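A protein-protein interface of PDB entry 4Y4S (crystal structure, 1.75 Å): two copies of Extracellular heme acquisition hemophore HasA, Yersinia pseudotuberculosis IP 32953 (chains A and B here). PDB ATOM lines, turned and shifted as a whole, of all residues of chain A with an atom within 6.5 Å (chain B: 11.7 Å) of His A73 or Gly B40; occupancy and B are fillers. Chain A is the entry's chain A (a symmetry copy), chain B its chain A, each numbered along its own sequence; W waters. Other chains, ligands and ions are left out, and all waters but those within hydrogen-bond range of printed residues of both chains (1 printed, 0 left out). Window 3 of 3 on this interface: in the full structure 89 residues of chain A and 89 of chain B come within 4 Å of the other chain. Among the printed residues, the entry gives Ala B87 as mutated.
The side-chain hydroxyl of Ser A72 sits at hydrogen-bond distance from the backbone carbonyl oxygen of Thr B60 (3.5 Å).
ND1 of His A73 lies close to O of Gly B40 (3.0 Å).
O of Phe B39 lies close to OG of Ser A71 (3.4 Å).
The side-chain carboxylate (OE1) of Glu A77 sits close to the backbone NH (N) of Phe B39 (3.2 Å).
OE1 of Glu A77 lies close to O of Trp B35 (2.6 Å).
O of Leu A158 sits close to O of Ala B36, at 3.3 Å.
O of Glu A77 is in hydrogen-bond range of N of Ser A71 (3.0 Å).
O of Lys B86 lies close to O of Leu B61 (2.7 Å).
Among the printed residues, merely in contact across the chains: His A73 with Phe B39 (3.9 Å), Glu A77 with Asn B38 (3.1 Å), Leu A158 with Trp B35 (3.9 Å), Met A159 with Phe B39 (3.9 Å) and Met A159 with Leu B61 (3.5 Å).
Of chain B, only Phe B39 (3.9 Å) and Gly B40 (2.9 Å) come within 4 Å of His A73.
Of chain A, only His A73 (2.9 Å) comes within 4 Å of Gly B40.
Of chain B, only Thr B60 comes within 4 Å of Ser A72.
No residue of chain B comes within 4 Å of Ser A74.
Pro A76 touches none of the printed residues of chain B.
Glu A77 touches just these residues of chain B: Trp B35, Asn B38 and Phe B39.
Of the printed residues of chain B, Leu A158 touches Trp B35 and Ala B36.
Printed residues of chain A within 4 Å of Thr B60: Ser A72 (3.5 Å).
Of the printed residues of chain A, Leu B61 touches Met A159 (3.5 Å).
Of the printed residues of chain A, Ala B36 touches Leu A158.
Arg B33 touches none of the printed residues of chain A.
The nearest residue of chain B that does not touch His A73 is Asn B38 (5.4 Å).
The nearest residue of chain A that does not touch Gly B40 is Met A159 (4.6 Å).
Of the 9 printed residues of chain A, 6 touch a printed residue of chain B.
Hydrophobic or aromatic side chains of chain A within 4 Å of the printed part of chain B: His A73, Leu A158 and Met A159.
Of the 17 printed residues of chain B, 7 touch a printed residue of chain A.
Printed residues of chain B that touch a printed residue of chain A: Trp B35, Ala B36, Asn B38, Phe B39, Gly B40, Thr B60 and Leu B61.
Hydrophobic or aromatic side chains of chain B that line the printed part of chain A: Trp B35, Ala B36, Phe B39 and Leu B61.
No position is printed for both chains.
Water W1 lies within hydrogen-bond range of OG of Ser A71 (2.5 Å), N of Glu A77 (2.8 Å), O of Phe B39 (3.1 Å) and O of Asn B38 (3.4 Å).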
ATOM      1  N   SER A  71       6.285 -25.579  26.507  1.00  0.00           N
ATOM      2  CA  SER A  71       7.283 -26.248  27.352  1.00  0.00           C
ATOM      3  C   SER A  71       8.640 -25.544  27.222  1.00  0.00           C
ATOM      4  O   SER A  71       8.772 -24.584  26.453  1.00  0.00           O
ATOM      5  CB  SER A  71       7.406 -27.737  26.993  1.00  0.00           C
ATOM      6  OG  SER A  71       8.150 -27.928  25.807  1.00  0.00           O
ATOM      7  N   SER A  72       9.643 -26.031  27.956  1.00  0.00           N
ATOM      8  CA  SER A  72      10.974 -25.409  27.954  1.00  0.00           C
ATOM      9  C   SER A  72      12.027 -26.213  27.180  1.00  0.00           C
ATOM     10  O   SER A  72      13.202 -25.871  27.186  1.00  0.00           O
ATOM     11  CB  SER A  72      11.453 -25.201  29.391  1.00  0.00           C
ATOM     12  OG  SER A  72      11.604 -26.454  30.032  1.00  0.00           O
ATOM     13  N   HIS A  73      11.599 -27.275  26.508  1.00  0.00           N
ATOM     14  CA  HIS A  73      12.517 -28.149  25.785  1.00  0.00           C
ATOM     15  C   HIS A  73      12.686 -27.663  24.348  1.00  0.00           C
ATOM     16  O   HIS A  73      11.992 -26.744  23.926  1.00  0.00           O
ATOM     17  CB  HIS A  73      12.008 -29.586  25.850  1.00  0.00           C
ATOM     18  CG  HIS A  73      11.852 -30.086  27.255  1.00  0.00           C
ATOM     19  ND1 HIS A  73      11.252 -31.289  27.566  1.00  0.00           N
ATOM     20  CD2 HIS A  73      12.217 -29.532  28.437  1.00  0.00           C
ATOM     21  CE1 HIS A  73      11.258 -31.454  28.879  1.00  0.00           C
ATOM     22  NE2 HIS A  73      11.833 -30.401  29.431  1.00  0.00           N
ATOM     23  N   SER A  74      13.617 -28.230  23.590  1.00  0.00           N
ATOM     24  CA  SER A  74      13.817 -27.686  22.246  1.00  0.00           C
ATOM     25  C   SER A  74      12.643 -28.140  21.411  1.00  0.00           C
ATOM     26  O   SER A  74      12.024 -29.156  21.732  1.00  0.00           O
ATOM     27  CB  SER A  74      15.133 -28.140  21.628  1.00  0.00           C
ATOM     28  OG  SER A  74      15.133 -29.539  21.428  1.00  0.00           O
ATOM     29  N   ASN A  75      12.334 -27.391  20.353  1.00  0.00           N
ATOM     30  CA  ASN A  75      11.118 -27.628  19.581  1.00  0.00           C
ATOM     31  C   ASN A  75       9.919 -27.806  20.528  1.00  0.00           C
ATOM     32  O   ASN A  75       9.239 -28.823  20.512  1.00  0.00           O
ATOM     33  CB  ASN A  75      11.308 -28.851  18.681  1.00  0.00           C
ATOM     34  CG  ASN A  75      10.305 -28.906  17.564  1.00  0.00           C
ATOM     35  OD1 ASN A  75       9.889 -29.987  17.150  1.00  0.00           O
ATOM     36  ND2 ASN A  75       9.912 -27.738  17.054  1.00  0.00           N
ATOM     37  N   PRO A  76       9.678 -26.814  21.384  1.00  0.00           N
ATOM     38  CA  PRO A  76       8.769 -27.077  22.503  1.00  0.00           C
ATOM     39  C   PRO A  76       7.329 -27.235  22.027  1.00  0.00           C
ATOM     40  O   PRO A  76       6.883 -26.512  21.130  1.00  0.00           O
ATOM     41  CB  PRO A  76       8.921 -25.831  23.388  1.00  0.00           C
ATOM     42  CG  PRO A  76       9.325 -24.749  22.401  1.00  0.00           C
ATOM     43  CD  PRO A  76      10.145 -25.413  21.341  1.00  0.00           C
ATOM     44  N   GLU A  77       6.613 -28.185  22.616  1.00  0.00           N
ATOM     45  CA  GLU A  77       5.175 -28.279  22.382  1.00  0.00           C
ATOM     46  C   GLU A  77       4.493 -27.077  22.994  1.00  0.00           C
ATOM     47  O   GLU A  77       4.922 -26.592  24.047  1.00  0.00           O
ATOM     48  CB  GLU A  77       4.594 -29.531  22.981  1.00  0.00           C
ATOM     49  CG  GLU A  77       4.979 -30.758  22.225  1.00  0.00           C
ATOM     50  CD  GLU A  77       4.267 -31.963  22.778  1.00  0.00           C
ATOM     51  OE1 GLU A  77       3.710 -31.871  23.902  1.00  0.00           O
ATOM     52  OE2 GLU A  77       4.282 -33.000  22.108  1.00  0.00           O
ATOM     53  N   LEU A 158      -2.638 -32.558  30.944  1.00  0.00           N
ATOM     54  CA  LEU A 158      -1.918 -32.606  29.703  1.00  0.00           C
ATOM     55  C   LEU A 158      -0.410 -32.444  29.929  1.00  0.00           C
ATOM     56  O   LEU A 158       0.427 -33.145  29.361  1.00  0.00           O
ATOM     57  CB  LEU A 158      -2.462 -31.517  28.765  1.00  0.00           C
ATOM     58  CG  LEU A 158      -3.704 -31.914  27.961  1.00  0.00           C
ATOM     59  CD1 LEU A 158      -4.162 -30.754  27.094  1.00  0.00           C
ATOM     60  CD2 LEU A 158      -3.420 -33.107  27.098  1.00  0.00           C
ATOM     61  N   MET A 159      -0.078 -31.514  30.797  1.00  0.00           N
ATOM     62  CA  MET A 159       1.307 -31.188  31.074  1.00  0.00           C
ATOM     63  C   MET A 159       2.042 -32.305  31.782  1.00  0.00           C
ATOM     64  O   MET A 159       3.280 -32.377  31.719  1.00  0.00           O
ATOM     65  CB  MET A 159       1.354 -29.902  31.893  1.00  0.00           C
ATOM     66  CG  MET A 159       0.702 -28.783  31.119  1.00  0.00           C
ATOM     67  SD  MET A 159       0.523 -27.277  32.051  1.00  0.00           S
ATOM     68  CE  MET A 159       2.259 -26.965  32.342  1.00  0.00           C
ATOM     69  N   LEU B  32      -3.659 -36.475  21.574  1.00  0.00           N
ATOM     70  CA  LEU B  32      -3.456 -35.736  22.805  1.00  0.00           C
ATOM     71  C   LEU B  32      -2.613 -36.595  23.760  1.00  0.00           C
ATOM     72  O   LEU B  32      -1.827 -36.048  24.550  1.00  0.00           O
ATOM     73  CB  LEU B  32      -4.776 -35.331  23.436  1.00  0.00           C
ATOM     74  CG  LEU B  32      -5.535 -34.158  22.809  1.00  0.00           C
ATOM     75  CD1 LEU B  32      -6.879 -33.953  23.589  1.00  0.00           C
ATOM     76  CD2 LEU B  32      -4.620 -32.850  22.757  1.00  0.00           C
ATOM     77  N   ARG B  33      -2.732 -37.927  23.666  1.00  0.00           N
ATOM     78  CA  ARG B  33      -1.901 -38.740  24.554  1.00  0.00           C
ATOM     79  C   ARG B  33      -0.426 -38.559  24.211  1.00  0.00           C
ATOM     80  O   ARG B  33       0.413 -38.369  25.086  1.00  0.00           O
ATOM     81  CB  ARG B  33      -2.264 -40.243  24.502  1.00  0.00           C
ATOM     82  CG  ARG B  33      -1.634 -40.920  25.755  1.00  0.00           C
ATOM     83  CD  ARG B  33      -2.230 -42.204  26.203  1.00  0.00           C
ATOM     84  NE  ARG B  33      -3.661 -42.195  26.537  1.00  0.00           N
ATOM     85  CZ  ARG B  33      -4.159 -42.074  27.768  1.00  0.00           C
ATOM     86  NH1 ARG B  33      -3.353 -41.860  28.820  1.00  0.00           N
ATOM     87  NH2 ARG B  33      -5.473 -42.151  27.947  1.00  0.00           N
ATOM     88  N   GLU B  34      -0.128 -38.606  22.921  1.00  0.00           N
ATOM     89  CA  GLU B  34       1.226 -38.335  22.449  1.00  0.00           C
ATOM     90  C   GLU B  34       1.683 -36.928  22.813  1.00  0.00           C
ATOM     91  O   GLU B  34       2.785 -36.755  23.269  1.00  0.00           O
ATOM     92  CB  GLU B  34       1.317 -38.513  20.942  1.00  0.00           C
ATOM     93  CG  GLU B  34       2.753 -38.292  20.374  1.00  0.00           C
ATOM     94  CD  GLU B  34       2.837 -38.534  18.864  1.00  0.00           C
ATOM     95  OE1 GLU B  34       2.537 -39.668  18.420  1.00  0.00           O
ATOM     96  OE2 GLU B  34       3.174 -37.588  18.116  1.00  0.00           O
ATOM     97  N   TRP B  35       0.867 -35.914  22.530  1.00  0.00           N
ATOM     98  CA  TRP B  35       1.230 -34.539  22.920  1.00  0.00           C
ATOM     99  C   TRP B  35       1.482 -34.451  24.431  1.00  0.00           C
ATOM    100  O   TRP B  35       2.491 -33.902  24.860  1.00  0.00           O
ATOM    101  CB  TRP B  35       0.121 -33.568  22.484  1.00  0.00           C
ATOM    102  CG  TRP B  35       0.473 -32.096  22.552  1.00  0.00           C
ATOM    103  CD1 TRP B  35       0.963 -31.314  21.538  1.00  0.00           C
ATOM    104  CD2 TRP B  35       0.325 -31.242  23.685  1.00  0.00           C
ATOM    105  NE1 TRP B  35       1.149 -30.017  21.992  1.00  0.00           N
ATOM    106  CE2 TRP B  35       0.775 -29.951  23.305  1.00  0.00           C
ATOM    107  CE3 TRP B  35      -0.110 -31.440  25.003  1.00  0.00           C
ATOM    108  CZ2 TRP B  35       0.768 -28.871  24.187  1.00  0.00           C
ATOM    109  CZ3 TRP B  35      -0.104 -30.371  25.874  1.00  0.00           C
ATOM    110  CH2 TRP B  35       0.338 -29.103  25.469  1.00  0.00           C
ATOM    111  N   ALA B  36       0.576 -35.003  25.233  1.00  0.00           N
ATOM    112  CA  ALA B  36       0.732 -34.975  26.676  1.00  0.00           C
ATOM    113  C   ALA B  36       2.044 -35.610  27.103  1.00  0.00           C
ATOM    114  O   ALA B  36       2.725 -35.083  27.968  1.00  0.00           O
ATOM    115  CB  ALA B  36      -0.430 -35.688  27.360  1.00  0.00           C
ATOM    116  N   ASN B  37       2.370 -36.757  26.528  1.00  0.00           N
ATOM    117  CA  ASN B  37       3.575 -37.489  26.929  1.00  0.00           C
ATOM    118  C   ASN B  37       4.859 -36.807  26.450  1.00  0.00           C
ATOM    119  O   ASN B  37       5.907 -37.013  27.036  1.00  0.00           O
ATOM    120  CB  ASN B  37       3.529 -38.955  26.415  1.00  0.00           C
ATOM    121  CG  ASN B  37       2.673 -39.895  27.317  1.00  0.00           C
ATOM    122  OD1 ASN B  37       3.209 -40.574  28.197  1.00  0.00           O
ATOM    123  ND2 ASN B  37       1.359 -39.930  27.096  1.00  0.00           N
ATOM    124  N   ASN B  38       4.795 -36.012  25.385  1.00  0.00           N
ATOM    125  CA  ASN B  38       5.991 -35.332  24.875  1.00  0.00           C
ATOM    126  C   ASN B  38       6.136 -33.907  25.325  1.00  0.00           C
ATOM    127  O   ASN B  38       6.989 -33.217  24.811  1.00  0.00           O
ATOM    128  CB  ASN B  38       6.013 -35.323  23.342  1.00  0.00           C
ATOM    129  CG  ASN B  38       6.312 -36.683  22.759  1.00  0.00           C
ATOM    130  OD1 ASN B  38       6.810 -37.560  23.450  1.00  0.00           O
ATOM    131  ND2 ASN B  38       6.015 -36.861  21.470  1.00  0.00           N
ATOM    132  N   PHE B  39       5.287 -33.458  26.245  1.00  0.00           N
ATOM    133  CA  PHE B  39       5.317 -32.082  26.700  1.00  0.00           C
ATOM    134  C   PHE B  39       6.559 -31.820  27.542  1.00  0.00           C
ATOM    135  O   PHE B  39       7.335 -30.934  27.225  1.00  0.00           O
ATOM    136  CB  PHE B  39       4.090 -31.735  27.523  1.00  0.00           C
ATOM    137  CG  PHE B  39       3.951 -30.253  27.820  1.00  0.00           C
ATOM    138  CD1 PHE B  39       3.372 -29.397  26.890  1.00  0.00           C
ATOM    139  CD2 PHE B  39       4.416 -29.717  29.006  1.00  0.00           C
ATOM    140  CE1 PHE B  39       3.264 -28.029  27.135  1.00  0.00           C
ATOM    141  CE2 PHE B  39       4.296 -28.349  29.280  1.00  0.00           C
ATOM    142  CZ  PHE B  39       3.711 -27.497  28.337  1.00  0.00           C
ATOM    143  N   GLY B  40       6.698 -32.575  28.634  1.00  0.00           N
ATOM    144  CA  GLY B  40       7.779 -32.383  29.580  1.00  0.00           C
ATOM    145  C   GLY B  40       8.851 -33.422  29.398  1.00  0.00           C
ATOM    146  O   GLY B  40       9.384 -33.562  28.297  1.00  0.00           O
ATOM    147  N   SER B  59       5.791 -24.551  36.784  1.00  0.00           N
ATOM    148  CA  SER B  59       6.975 -25.460  36.923  1.00  0.00           C
ATOM    149  C   SER B  59       6.969 -26.606  35.874  1.00  0.00           C
ATOM    150  O   SER B  59       6.155 -27.528  36.006  1.00  0.00           O
ATOM    151  CB  SER B  59       7.071 -26.096  38.328  1.00  0.00           C
ATOM    152  OG  SER B  59       7.832 -27.302  38.340  1.00  0.00           O
ATOM    153  N   THR B  60       7.833 -26.591  34.842  1.00  0.00           N
ATOM    154  CA  THR B  60       8.773 -25.514  34.483  1.00  0.00           C
ATOM    155  C   THR B  60       8.438 -24.905  33.093  1.00  0.00           C
ATOM    156  O   THR B  60       9.081 -25.208  32.067  1.00  0.00           O
ATOM    157  CB  THR B  60      10.240 -26.017  34.464  1.00  0.00           C
ATOM    158  OG1 THR B  60      11.042 -25.157  33.636  1.00  0.00           O
ATOM    159  CG2 THR B  60      10.328 -27.448  33.924  1.00  0.00           C
ATOM    160  N   LEU B  61       7.445 -24.027  33.055  1.00  0.00           N
ATOM    161  CA  LEU B  61       6.782 -23.773  31.791  1.00  0.00           C
ATOM    162  C   LEU B  61       6.861 -22.334  31.286  1.00  0.00           C
ATOM    163  O   LEU B  61       7.181 -21.394  32.020  1.00  0.00           O
ATOM    164  CB  LEU B  61       5.313 -24.227  31.897  1.00  0.00           C
ATOM    165  CG  LEU B  61       4.309 -23.381  32.676  1.00  0.00           C
ATOM    166  CD1 LEU B  61       3.273 -22.803  31.728  1.00  0.00           C
ATOM    167  CD2 LEU B  61       3.628 -24.143  33.798  1.00  0.00           C
ATOM    168  N   PHE B  62       6.595 -22.192  29.997  1.00  0.00           N
ATOM    169  CA  PHE B  62       6.391 -20.896  29.360  1.00  0.00           C
ATOM    170  C   PHE B  62       4.899 -20.631  29.241  1.00  0.00           C
ATOM    171  O   PHE B  62       4.156 -21.455  28.691  1.00  0.00           O
ATOM    172  CB  PHE B  62       7.033 -20.865  27.986  1.00  0.00           C
ATOM    173  CG  PHE B  62       6.818 -19.570  27.267  1.00  0.00           C
ATOM    174  CD1 PHE B  62       7.352 -18.382  27.775  1.00  0.00           C
ATOM    175  CD2 PHE B  62       6.086 -19.526  26.085  1.00  0.00           C
ATOM    176  CE1 PHE B  62       7.160 -17.171  27.122  1.00  0.00           C
ATOM    177  CE2 PHE B  62       5.887 -18.308  25.420  1.00  0.00           C
ATOM    178  CZ  PHE B  62       6.428 -17.131  25.945  1.00  0.00           C
ATOM    179  N   SER B  63       4.442 -19.519  29.797  1.00  0.00           N
ATOM    180  CA  SER B  63       3.022 -19.189  29.740  1.00  0.00           C
ATOM    181  C   SER B  63       2.819 -17.725  29.310  1.00  0.00           C
ATOM    182  O   SER B  63       3.635 -16.885  29.645  1.00  0.00           O
ATOM    183  CB  SER B  63       2.384 -19.429  31.098  1.00  0.00           C
ATOM    184  OG  SER B  63       1.218 -18.649  31.228  1.00  0.00           O
ATOM    185  N   LEU B  85       5.736 -15.353  30.781  1.00  0.00           N
ATOM    186  CA  LEU B  85       6.467 -15.788  31.962  1.00  0.00           C
ATOM    187  C   LEU B  85       7.101 -17.182  31.815  1.00  0.00           C
ATOM    188  O   LEU B  85       6.505 -18.077  31.175  1.00  0.00           O
ATOM    189  CB  LEU B  85       5.527 -15.821  33.164  1.00  0.00           C
ATOM    190  CG  LEU B  85       6.069 -16.466  34.443  1.00  0.00           C
ATOM    191  CD1 LEU B  85       7.082 -15.561  35.157  1.00  0.00           C
ATOM    192  CD2 LEU B  85       4.941 -16.930  35.377  1.00  0.00           C
ATOM    193  N   LYS B  86       8.284 -17.335  32.437  1.00  0.00           N
ATOM    194  CA  LYS B  86       8.874 -18.616  32.900  1.00  0.00           C
ATOM    195  C   LYS B  86       8.092 -19.367  34.009  1.00  0.00           C
ATOM    196  O   LYS B  86       6.874 -19.540  33.909  1.00  0.00           O
ATOM    197  CB  LYS B  86      10.298 -18.375  33.405  1.00  0.00           C
ATOM    198  CG  LYS B  86      11.339 -18.434  32.308  1.00  0.00           C
ATOM    199  CD  LYS B  86      10.703 -18.810  30.974  1.00  0.00           C
ATOM    200  CE  LYS B  86      11.712 -19.423  30.011  1.00  0.00           C
ATOM    201  NZ  LYS B  86      11.075 -19.782  28.707  1.00  0.00           N
ATOM    202  N   ALA B  87       8.768 -19.806  35.075  1.00  0.00           N
ATOM    203  CA  ALA B  87       8.227 -20.962  35.808  1.00  0.00           C
ATOM    204  C   ALA B  87       8.336 -21.085  37.339  1.00  0.00           C
ATOM    205  O   ALA B  87       9.437 -21.344  37.841  1.00  0.00           O
ATOM    206  CB  ALA B  87       8.851 -22.195  35.214  1.00  0.00           C
HETATM  207  O   HOH W   1       7.895 -29.993  24.370  1.00  0.00           O
